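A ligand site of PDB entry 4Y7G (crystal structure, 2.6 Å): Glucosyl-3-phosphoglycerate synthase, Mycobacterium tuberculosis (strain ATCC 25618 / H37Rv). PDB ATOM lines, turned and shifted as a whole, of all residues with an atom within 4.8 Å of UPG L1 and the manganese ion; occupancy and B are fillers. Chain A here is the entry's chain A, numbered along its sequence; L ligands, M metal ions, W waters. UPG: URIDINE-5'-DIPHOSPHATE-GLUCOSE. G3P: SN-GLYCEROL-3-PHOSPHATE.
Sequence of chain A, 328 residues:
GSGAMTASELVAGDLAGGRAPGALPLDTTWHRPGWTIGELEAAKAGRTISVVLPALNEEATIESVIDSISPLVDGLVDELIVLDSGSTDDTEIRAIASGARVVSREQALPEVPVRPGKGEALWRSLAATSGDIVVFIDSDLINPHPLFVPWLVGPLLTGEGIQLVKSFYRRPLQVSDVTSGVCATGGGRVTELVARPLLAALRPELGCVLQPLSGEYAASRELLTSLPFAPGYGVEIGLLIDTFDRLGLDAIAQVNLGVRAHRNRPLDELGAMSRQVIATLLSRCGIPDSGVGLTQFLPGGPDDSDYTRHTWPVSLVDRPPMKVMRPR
The manganese ion is bound by a ring nitrogen (ND1) of His 262, water W3, water W5, an oxygen (O1A) of UPG L1, the side-chain carboxylate (OD2) of Asp 140 and an oxygen (O2B) of UPG L1. The manganese ion has six donor atoms within binding distance.
Water W5 lies within hydrogen-bond range of O of Arg 263 and O1B of UPG L1. Water W3 lies within hydrogen-bond range of OD2 of Asp 138 (2.7 Å), O2' of UPG L1 (3.2 Å) and NH1 of Arg 260 (3.3 Å). Water W2 bridges an oxygen (O4) of UPG L1 (2.9 Å) and the backbone NH (N) of Gly 117 (3.2 Å). Water W4 lies within hydrogen-bond range of O of Tyr 233 (2.8 Å), O6' of UPG L1 (3.0 Å) and N of Glu 236 (3.1 Å).
Two residues have an atom within 4 Å of the manganese ion: Asp 140 and His 262.
An oxygen (O3B) of UPG L1 sits close to the side-chain sulfur of Met 273, 3.4 Å away. Merely in contact with UPG L1: Gly 117 (3.4 Å), Leu 213 (3.5 Å) and Gly 215 (3.4 Å). Hydrophobic or aromatic side chains that line UPG L1: Pro 54, Leu 56, Leu 213, Tyr 233, His 262 and Met 273. Of the 24 residues printed, 18 come within 4 Å of UPG L1. The nearest printed residue that does not touch UPG L1 is Ala 121 (4.4 Å).
An oxygen (O4) of UPG L1 lies within hydrogen-bond range of the backbone NH of Lys 118, 3.4 Å away. O3' of UPG L1 is in hydrogen-bond range of NZ of Lys 118 (2.4 Å). OE2 of Glu 236 lies within hydrogen-bond range of O4' of UPG L1, 2.4 Å away. The backbone NH of Leu 56 is in hydrogen-bond range of an oxygen (O2C) of UPG L1. OH of Tyr 233 lies within hydrogen-bond range of O2A of UPG L1 (3.0 Å). The side-chain carboxylate (OD2) of Asp 138 lies within hydrogen-bond range of an oxygen (O2') of UPG L1 (3.0 Å). NH1 of Arg 260 is in hydrogen-bond range of O2' of UPG L1. An oxygen (O3C) of UPG L1 lies within hydrogen-bond range of the backbone NH (N) of Ser 139 (3.1 Å). The side-chain hydroxyl of Ser 139 sits at hydrogen-bond distance from an oxygen (O3C) of UPG L1, at 3.1 Å. The side-chain carboxylate (OE2) of Glu 58 is in hydrogen-bond range of an oxygen (O2C) of UPG L1 (3.1 Å). OG of Ser 85 sits at hydrogen-bond distance from N3 of UPG L1 (3.1 Å). An oxygen (O1B) of UPG L1 lies within salt-bridge range of the guanidinium group (NH1) of Arg 265. The backbone carbonyl oxygen of Pro 54 sits at hydrogen-bond distance from an oxygen (O3C) of UPG L1, at 3.3 Å. The backbone NH (N) of Ala 55 lies within hydrogen-bond range of an oxygen (O2) of UPG L1 (3.4 Å). A ring nitrogen (NE2) of His 262 is in hydrogen-bond range of an oxygen (O2) of G3P L2, at 3.2 Å. The guanidinium group (NH2) of Arg 260 is in hydrogen-bond range of an oxygen (O2) of G3P L2.
N of Arg 263 sits close to OD2 of Asp 140. The side-chain amino group (NZ) of Lys 118 is in salt-bridge range of the side-chain carboxylate (OE1) of Glu 236. The side-chain carboxylate of Asp 138 is in salt-bridge range of the side-chain amino group of Lys 118 (3.1 Å). The side-chain hydroxyl (OH) of Tyr 233 sits at hydrogen-bond distance from the guanidinium group (NH2) of Arg 265. The side-chain carboxylate (OD2) of Asp 138 is in salt-bridge range of the guanidinium group (NH1) of Arg 260, 3.0 Å away. The side-chain hydroxyl of Ser 139 is in hydrogen-bond range of the backbone carbonyl oxygen of Pro 54. The side-chain carboxylate (OE1) of Glu 58 lies within salt-bridge range of the guanidinium group (NH2) of Arg 263, 2.5 Å away. The backbone NH (N) of Ser 85 is in hydrogen-bond range of the backbone carbonyl oxygen (O) of Ala 55 (2.8 Å).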
ATOM      1  N   PRO A  54       5.715 -16.872  16.298  1.00  0.00           N
ATOM      2  CA  PRO A  54       7.121 -16.473  16.170  1.00  0.00           C
ATOM      3  C   PRO A  54       7.211 -15.242  15.299  1.00  0.00           C
ATOM      4  O   PRO A  54       6.453 -15.157  14.316  1.00  0.00           O
ATOM      5  CB  PRO A  54       7.777 -17.693  15.519  1.00  0.00           C
ATOM      6  CG  PRO A  54       6.678 -18.294  14.696  1.00  0.00           C
ATOM      7  CD  PRO A  54       5.402 -18.077  15.500  1.00  0.00           C
ATOM      8  N   ALA A  55       8.129 -14.323  15.558  1.00  0.00           N
ATOM      9  CA  ALA A  55       8.153 -13.131  14.738  1.00  0.00           C
ATOM     10  C   ALA A  55       9.540 -12.565  14.592  1.00  0.00           C
ATOM     11  O   ALA A  55      10.255 -12.337  15.576  1.00  0.00           O
ATOM     12  CB  ALA A  55       7.217 -12.080  15.326  1.00  0.00           C
ATOM     13  N   LEU A  56       9.943 -12.363  13.345  1.00  0.00           N
ATOM     14  CA  LEU A  56      11.161 -11.656  13.042  1.00  0.00           C
ATOM     15  C   LEU A  56      10.842 -10.585  12.019  1.00  0.00           C
ATOM     16  O   LEU A  56      10.631 -10.894  10.846  1.00  0.00           O
ATOM     17  CB  LEU A  56      12.221 -12.634  12.511  1.00  0.00           C
ATOM     18  CG  LEU A  56      13.544 -12.009  12.088  1.00  0.00           C
ATOM     19  CD1 LEU A  56      14.152 -11.188  13.221  1.00  0.00           C
ATOM     20  CD2 LEU A  56      14.477 -13.094  11.649  1.00  0.00           C
ATOM     21  N   GLU A  58       8.119  -8.492  11.482  1.00  0.00           N
ATOM     22  CA  GLU A  58       6.804  -8.561  10.840  1.00  0.00           C
ATOM     23  C   GLU A  58       5.861  -7.418  11.283  1.00  0.00           C
ATOM     24  O   GLU A  58       4.665  -7.648  11.484  1.00  0.00           O
ATOM     25  CB  GLU A  58       6.174  -9.930  11.128  1.00  0.00           C
ATOM     26  CG  GLU A  58       7.077 -11.125  10.782  1.00  0.00           C
ATOM     27  CD  GLU A  58       7.371 -11.276   9.290  1.00  0.00           C
ATOM     28  OE1 GLU A  58       7.069 -10.355   8.511  1.00  0.00           O
ATOM     29  OE2 GLU A  58       7.912 -12.315   8.875  1.00  0.00           O
ATOM     30  N   SER A  85      11.903 -12.758  17.802  1.00  0.00           N
ATOM     31  CA  SER A  85      13.087 -13.509  17.466  1.00  0.00           C
ATOM     32  C   SER A  85      14.232 -12.585  17.052  1.00  0.00           C
ATOM     33  O   SER A  85      14.916 -12.845  16.068  1.00  0.00           O
ATOM     34  CB  SER A  85      12.736 -14.507  16.357  1.00  0.00           C
ATOM     35  OG  SER A  85      13.875 -15.201  15.909  1.00  0.00           O
ATOM     36  N   GLY A 117      17.566 -18.368  14.058  1.00  0.00           N
ATOM     37  CA  GLY A 117      16.675 -19.165  13.224  1.00  0.00           C
ATOM     38  C   GLY A 117      15.343 -19.451  13.876  1.00  0.00           C
ATOM     39  O   GLY A 117      15.155 -19.296  15.083  1.00  0.00           O
ATOM     40  N   LYS A 118      14.395 -19.869  13.042  1.00  0.00           N
ATOM     41  CA  LYS A 118      13.045 -20.086  13.490  1.00  0.00           C
ATOM     42  C   LYS A 118      12.961 -21.222  14.504  1.00  0.00           C
ATOM     43  O   LYS A 118      12.276 -21.099  15.515  1.00  0.00           O
ATOM     44  CB  LYS A 118      12.140 -20.367  12.308  1.00  0.00           C
ATOM     45  CG  LYS A 118      10.673 -20.204  12.647  1.00  0.00           C
ATOM     46  CD  LYS A 118       9.829 -20.757  11.555  1.00  0.00           C
ATOM     47  CE  LYS A 118       8.371 -20.761  12.005  1.00  0.00           C
ATOM     48  NZ  LYS A 118       7.435 -21.413  11.031  1.00  0.00           N
ATOM     49  N   ALA A 121      13.510 -20.317  17.973  1.00  0.00           N
ATOM     50  CA  ALA A 121      12.424 -19.533  18.550  1.00  0.00           C
ATOM     51  C   ALA A 121      11.309 -20.437  19.024  1.00  0.00           C
ATOM     52  O   ALA A 121      10.805 -20.279  20.125  1.00  0.00           O
ATOM     53  CB  ALA A 121      11.918 -18.560  17.522  1.00  0.00           C
ATOM     54  N   ASP A 138       2.202 -18.356  11.951  1.00  0.00           N
ATOM     55  CA  ASP A 138       3.191 -17.389  11.503  1.00  0.00           C
ATOM     56  C   ASP A 138       2.630 -15.989  11.644  1.00  0.00           C
ATOM     57  O   ASP A 138       1.438 -15.760  11.461  1.00  0.00           O
ATOM     58  CB  ASP A 138       3.593 -17.598  10.045  1.00  0.00           C
ATOM     59  CG  ASP A 138       4.480 -18.831   9.826  1.00  0.00           C
ATOM     60  OD1 ASP A 138       5.146 -19.343  10.757  1.00  0.00           O
ATOM     61  OD2 ASP A 138       4.495 -19.295   8.653  1.00  0.00           O
ATOM     62  N   SER A 139       3.515 -15.048  11.940  1.00  0.00           N
ATOM     63  CA  SER A 139       3.121 -13.671  12.199  1.00  0.00           C
ATOM     64  C   SER A 139       3.194 -12.813  10.926  1.00  0.00           C
ATOM     65  O   SER A 139       2.933 -11.606  10.973  1.00  0.00           O
ATOM     66  CB  SER A 139       3.972 -13.099  13.322  1.00  0.00           C
ATOM     67  OG  SER A 139       5.326 -13.262  13.047  1.00  0.00           O
ATOM     68  N   ASP A 140       3.566 -13.432   9.804  1.00  0.00           N
ATOM     69  CA  ASP A 140       3.619 -12.727   8.519  1.00  0.00           C
ATOM     70  C   ASP A 140       2.401 -12.988   7.638  1.00  0.00           C
ATOM     71  O   ASP A 140       2.376 -12.604   6.460  1.00  0.00           O
ATOM     72  CB  ASP A 140       4.877 -13.130   7.742  1.00  0.00           C
ATOM     73  CG  ASP A 140       4.742 -14.490   7.084  1.00  0.00           C
ATOM     74  OD1 ASP A 140       4.170 -15.415   7.716  1.00  0.00           O
ATOM     75  OD2 ASP A 140       5.230 -14.650   5.945  1.00  0.00           O
ATOM     76  N   LEU A 213       5.481 -28.113   5.063  1.00  0.00           N
ATOM     77  CA  LEU A 213       6.213 -26.931   5.528  1.00  0.00           C
ATOM     78  C   LEU A 213       5.302 -25.888   6.174  1.00  0.00           C
ATOM     79  O   LEU A 213       5.758 -24.814   6.540  1.00  0.00           O
ATOM     80  CB  LEU A 213       7.004 -26.298   4.374  1.00  0.00           C
ATOM     81  CG  LEU A 213       8.072 -27.196   3.734  1.00  0.00           C
ATOM     82  CD1 LEU A 213       8.945 -26.378   2.819  1.00  0.00           C
ATOM     83  CD2 LEU A 213       8.948 -28.000   4.769  1.00  0.00           C
ATOM     84  N   SER A 214       4.023 -26.197   6.336  1.00  0.00           N
ATOM     85  CA  SER A 214       3.126 -25.180   6.854  1.00  0.00           C
ATOM     86  C   SER A 214       3.525 -24.645   8.222  1.00  0.00           C
ATOM     87  O   SER A 214       3.845 -25.415   9.140  1.00  0.00           O
ATOM     88  CB  SER A 214       1.718 -25.741   6.958  1.00  0.00           C
ATOM     89  OG  SER A 214       0.841 -24.669   7.300  1.00  0.00           O
ATOM     90  N   GLY A 215       3.561 -23.323   8.334  1.00  0.00           N
ATOM     91  CA  GLY A 215       3.833 -22.672   9.602  1.00  0.00           C
ATOM     92  C   GLY A 215       2.693 -22.664  10.589  1.00  0.00           C
ATOM     93  O   GLY A 215       2.875 -22.257  11.740  1.00  0.00           O
ATOM     94  N   TYR A 233      14.980 -22.859   9.280  1.00  0.00           N
ATOM     95  CA  TYR A 233      13.784 -23.345   8.584  1.00  0.00           C
ATOM     96  C   TYR A 233      13.626 -24.878   8.519  1.00  0.00           C
ATOM     97  O   TYR A 233      12.751 -25.373   7.806  1.00  0.00           O
ATOM     98  CB  TYR A 233      13.746 -22.763   7.178  1.00  0.00           C
ATOM     99  CG  TYR A 233      13.541 -21.267   7.189  1.00  0.00           C
ATOM    100  CD1 TYR A 233      12.362 -20.706   7.671  1.00  0.00           C
ATOM    101  CD2 TYR A 233      14.544 -20.410   6.755  1.00  0.00           C
ATOM    102  CE1 TYR A 233      12.171 -19.321   7.694  1.00  0.00           C
ATOM    103  CE2 TYR A 233      14.369 -19.040   6.778  1.00  0.00           C
ATOM    104  CZ  TYR A 233      13.182 -18.500   7.254  1.00  0.00           C
ATOM    105  OH  TYR A 233      13.018 -17.138   7.273  1.00  0.00           O
ATOM    106  N   VAL A 235      12.798 -26.730  11.016  1.00  0.00           N
ATOM    107  CA  VAL A 235      12.023 -27.144  12.167  1.00  0.00           C
ATOM    108  C   VAL A 235      10.723 -27.855  11.761  1.00  0.00           C
ATOM    109  O   VAL A 235      10.397 -28.872  12.369  1.00  0.00           O
ATOM    110  CB  VAL A 235      11.725 -25.947  13.097  1.00  0.00           C
ATOM    111  CG1 VAL A 235      10.930 -24.856  12.363  1.00  0.00           C
ATOM    112  CG2 VAL A 235      11.007 -26.389  14.331  1.00  0.00           C
ATOM    113  N   GLU A 236       9.978 -27.392  10.769  1.00  0.00           N
ATOM    114  CA  GLU A 236       8.729 -28.087  10.441  1.00  0.00           C
ATOM    115  C   GLU A 236       8.911 -29.481   9.903  1.00  0.00           C
ATOM    116  O   GLU A 236       8.303 -30.425  10.380  1.00  0.00           O
ATOM    117  CB  GLU A 236       7.901 -27.312   9.419  1.00  0.00           C
ATOM    118  CG  GLU A 236       7.141 -26.154  10.016  1.00  0.00           C
ATOM    119  CD  GLU A 236       8.031 -24.977  10.300  1.00  0.00           C
ATOM    120  OE1 GLU A 236       7.743 -24.249  11.282  1.00  0.00           O
ATOM    121  OE2 GLU A 236       9.002 -24.769   9.558  1.00  0.00           O
ATOM    122  N   ARG A 260      -4.091 -19.035   1.577  1.00  0.00           N
ATOM    123  CA  ARG A 260      -3.085 -18.317   2.338  1.00  0.00           C
ATOM    124  C   ARG A 260      -2.237 -17.383   1.540  1.00  0.00           C
ATOM    125  O   ARG A 260      -1.842 -17.632   0.407  1.00  0.00           O
ATOM    126  CB  ARG A 260      -2.144 -19.362   2.906  1.00  0.00           C
ATOM    127  CG  ARG A 260      -1.224 -18.985   4.035  1.00  0.00           C
ATOM    128  CD  ARG A 260       0.075 -19.780   3.890  1.00  0.00           C
ATOM    129  NE  ARG A 260       0.876 -19.811   5.122  1.00  0.00           N
ATOM    130  CZ  ARG A 260       2.195 -20.009   5.162  1.00  0.00           C
ATOM    131  NH1 ARG A 260       2.813 -20.021   6.340  1.00  0.00           N
ATOM    132  NH2 ARG A 260       2.882 -20.194   4.040  1.00  0.00           N
ATOM    133  N   HIS A 262       1.103 -14.565   2.277  1.00  0.00           N
ATOM    134  CA  HIS A 262       2.115 -14.150   3.237  1.00  0.00           C
ATOM    135  C   HIS A 262       3.182 -13.409   2.474  1.00  0.00           C
ATOM    136  O   HIS A 262       3.098 -13.279   1.253  1.00  0.00           O
ATOM    137  CB  HIS A 262       2.669 -15.332   4.050  1.00  0.00           C
ATOM    138  CG  HIS A 262       3.429 -16.324   3.249  1.00  0.00           C
ATOM    139  ND1 HIS A 262       4.632 -16.866   3.659  1.00  0.00           N
ATOM    140  CD2 HIS A 262       3.153 -16.894   2.053  1.00  0.00           C
ATOM    141  CE1 HIS A 262       5.064 -17.724   2.753  1.00  0.00           C
ATOM    142  NE2 HIS A 262       4.182 -17.752   1.763  1.00  0.00           N
ATOM    143  N   ARG A 263       4.186 -12.954   3.210  1.00  0.00           N
ATOM    144  CA  ARG A 263       5.342 -12.293   2.593  1.00  0.00           C
ATOM    145  C   ARG A 263       5.961 -13.197   1.541  1.00  0.00           C
ATOM    146  O   ARG A 263       6.266 -14.362   1.794  1.00  0.00           O
ATOM    147  CB  ARG A 263       6.371 -11.945   3.655  1.00  0.00           C
ATOM    148  CG  ARG A 263       7.542 -11.130   3.136  1.00  0.00           C
ATOM    149  CD  ARG A 263       8.690 -11.161   4.119  1.00  0.00           C
ATOM    150  NE  ARG A 263       8.348 -10.567   5.416  1.00  0.00           N
ATOM    151  CZ  ARG A 263       8.506  -9.288   5.712  1.00  0.00           C
ATOM    152  NH1 ARG A 263       8.997  -8.447   4.816  1.00  0.00           N
ATOM    153  NH2 ARG A 263       8.196  -8.847   6.910  1.00  0.00           N
ATOM    154  N   ARG A 265       9.187 -13.824  -0.198  1.00  0.00           N
ATOM    155  CA  ARG A 265      10.622 -13.689  -0.123  1.00  0.00           C
ATOM    156  C   ARG A 265      11.316 -13.806  -1.482  1.00  0.00           C
ATOM    157  O   ARG A 265      10.801 -14.470  -2.394  1.00  0.00           O
ATOM    158  CB  ARG A 265      11.131 -14.695   0.882  1.00  0.00           C
ATOM    159  CG  ARG A 265      10.392 -14.570   2.206  1.00  0.00           C
ATOM    160  CD  ARG A 265      10.780 -15.679   3.143  1.00  0.00           C
ATOM    161  NE  ARG A 265      12.165 -15.544   3.573  1.00  0.00           N
ATOM    162  CZ  ARG A 265      12.939 -16.558   3.910  1.00  0.00           C
ATOM    163  NH1 ARG A 265      12.482 -17.814   3.875  1.00  0.00           N
ATOM    164  NH2 ARG A 265      14.194 -16.310   4.287  1.00  0.00           N
ATOM    165  N   LEU A 270      15.025 -18.136  -0.364  1.00  0.00           N
ATOM    166  CA  LEU A 270      14.373 -19.436  -0.462  1.00  0.00           C
ATOM    167  C   LEU A 270      15.392 -20.510  -0.719  1.00  0.00           C
ATOM    168  O   LEU A 270      15.217 -21.644  -0.308  1.00  0.00           O
ATOM    169  CB  LEU A 270      13.344 -19.428  -1.592  1.00  0.00           C
ATOM    170  CG  LEU A 270      12.158 -18.474  -1.462  1.00  0.00           C
ATOM    171  CD1 LEU A 270      11.269 -18.634  -2.671  1.00  0.00           C
ATOM    172  CD2 LEU A 270      11.376 -18.713  -0.167  1.00  0.00           C
ATOM    173  N   MET A 273      16.714 -21.373   2.436  1.00  0.00           N
ATOM    174  CA  MET A 273      15.728 -22.050   3.262  1.00  0.00           C
ATOM    175  C   MET A 273      15.709 -23.515   2.849  1.00  0.00           C
ATOM    176  O   MET A 273      15.702 -24.423   3.666  1.00  0.00           O
ATOM    177  CB  MET A 273      14.350 -21.428   3.107  1.00  0.00           C
ATOM    178  CG  MET A 273      13.271 -22.264   3.736  1.00  0.00           C
ATOM    179  SD  MET A 273      11.693 -21.434   3.955  1.00  0.00           S
ATOM    180  CE  MET A 273      11.077 -21.327   2.308  1.00  0.00           C
ATOM    181  N   VAL A 277      16.270 -27.094   4.751  1.00  0.00           N
ATOM    182  CA  VAL A 277      15.214 -28.102   4.741  1.00  0.00           C
ATOM    183  C   VAL A 277      15.811 -29.439   4.311  1.00  0.00           C
ATOM    184  O   VAL A 277      15.513 -30.485   4.878  1.00  0.00           O
ATOM    185  CB  VAL A 277      14.061 -27.672   3.788  1.00  0.00           C
ATOM    186  CG1 VAL A 277      13.127 -28.827   3.469  1.00  0.00           C
ATOM    187  CG2 VAL A 277      13.300 -26.551   4.410  1.00  0.00           C
HETATM  188  N1  UPG L   1      10.779 -16.366  11.856  1.00  0.00           N
HETATM  189  C2  UPG L   1      11.423 -16.200  13.090  1.00  0.00           C
HETATM  190  N3  UPG L   1      12.761 -16.282  13.169  1.00  0.00           N
HETATM  191  C4  UPG L   1      13.513 -16.499  12.084  1.00  0.00           C
HETATM  192  C5  UPG L   1      12.898 -16.661  10.848  1.00  0.00           C
HETATM  193  C6  UPG L   1      11.518 -16.596  10.762  1.00  0.00           C
HETATM  194  O2  UPG L   1      10.742 -15.994  14.116  1.00  0.00           O
HETATM  195  O4  UPG L   1      14.763 -16.566  12.196  1.00  0.00           O
HETATM  196  C1C UPG L   1       9.314 -16.283  11.779  1.00  0.00           C
HETATM  197  C2C UPG L   1       8.814 -15.182  10.831  1.00  0.00           C
HETATM  198  O2C UPG L   1       8.545 -13.938  11.480  1.00  0.00           O
HETATM  199  C3C UPG L   1       7.555 -15.763  10.252  1.00  0.00           C
HETATM  200  C4C UPG L   1       7.699 -17.267  10.435  1.00  0.00           C
HETATM  201  O4C UPG L   1       8.816 -17.505  11.282  1.00  0.00           O
HETATM  202  O3C UPG L   1       6.419 -15.335  10.985  1.00  0.00           O
HETATM  203  C5C UPG L   1       7.929 -17.974   9.115  1.00  0.00           C
HETATM  204  O5C UPG L   1       9.070 -17.377   8.513  1.00  0.00           O
HETATM  205  PA  UPG L   1       9.041 -17.062   6.952  1.00  0.00           P
HETATM  206  O1A UPG L   1       7.760 -16.325   6.630  1.00  0.00           O
HETATM  207  O2A UPG L   1      10.277 -16.268   6.599  1.00  0.00           O
HETATM  208  O3A UPG L   1       9.050 -18.519   6.307  1.00  0.00           O
HETATM  209  PB  UPG L   1       8.415 -18.994   4.908  1.00  0.00           P
HETATM  210  O1B UPG L   1       9.190 -18.555   3.705  1.00  0.00           O
HETATM  211  O2B UPG L   1       6.929 -18.707   4.812  1.00  0.00           O
HETATM  212  O3B UPG L   1       8.642 -20.580   5.104  1.00  0.00           O
HETATM  213  C1' UPG L   1       7.618 -21.569   5.069  1.00  0.00           C
HETATM  214  C2' UPG L   1       6.708 -21.501   6.298  1.00  0.00           C
HETATM  215  C3' UPG L   1       7.594 -21.407   7.531  1.00  0.00           C
HETATM  216  C4' UPG L   1       8.470 -22.644   7.557  1.00  0.00           C
HETATM  217  C5' UPG L   1       9.236 -22.823   6.243  1.00  0.00           C
HETATM  218  C6' UPG L   1      10.023 -24.133   6.251  1.00  0.00           C
HETATM  219  O2' UPG L   1       5.783 -20.397   6.210  1.00  0.00           O
HETATM  220  O3' UPG L   1       6.790 -21.341   8.704  1.00  0.00           O
HETATM  221  O4' UPG L   1       9.429 -22.586   8.594  1.00  0.00           O
HETATM  222  O5' UPG L   1       8.320 -22.788   5.137  1.00  0.00           O
HETATM  223  O6' UPG L   1       9.248 -25.136   6.915  1.00  0.00           O
HETATM  224  O1  G3P L   2       6.383 -22.951   1.009  1.00  0.00           O
HETATM  225  C1  G3P L   2       5.425 -22.107   1.633  1.00  0.00           C
HETATM  226  C2  G3P L   2       4.481 -21.413   0.637  1.00  0.00           C
HETATM  227  O2  G3P L   2       3.394 -20.831   1.342  1.00  0.00           O
HETATM  228  C3  G3P L   2       5.308 -20.351  -0.127  1.00  0.00           C
HETATM  229  O1P G3P L   2       5.146 -20.253  -1.535  1.00  0.00           O
HETATM  230  O4P G3P L   2       4.808 -18.424  -3.342  1.00  0.00           O
HETATM  231  O2P G3P L   2       7.040 -19.389  -3.038  1.00  0.00           O
HETATM  232  O3P G3P L   2       6.154 -17.876  -1.339  1.00  0.00           O
HETATM  233  P   G3P L   2       5.786 -18.974  -2.321  1.00  0.00           P
HETATM  234 MN    MN M   1       6.116 -16.546   5.190  1.00  0.00          MN
HETATM  235  O   HOH W   1      17.141 -15.573  10.067  1.00  0.00           O
HETATM  236  O   HOH W   2      16.945 -15.263  13.597  1.00  0.00           O
HETATM  237  O   HOH W   3       4.792 -17.422   6.680  1.00  0.00           O
HETATM  238  O   HOH W   4      10.913 -27.473   7.798  1.00  0.00           O
HETATM  239  O   HOH W   5       7.677 -15.575   4.009  1.00  0.00           O
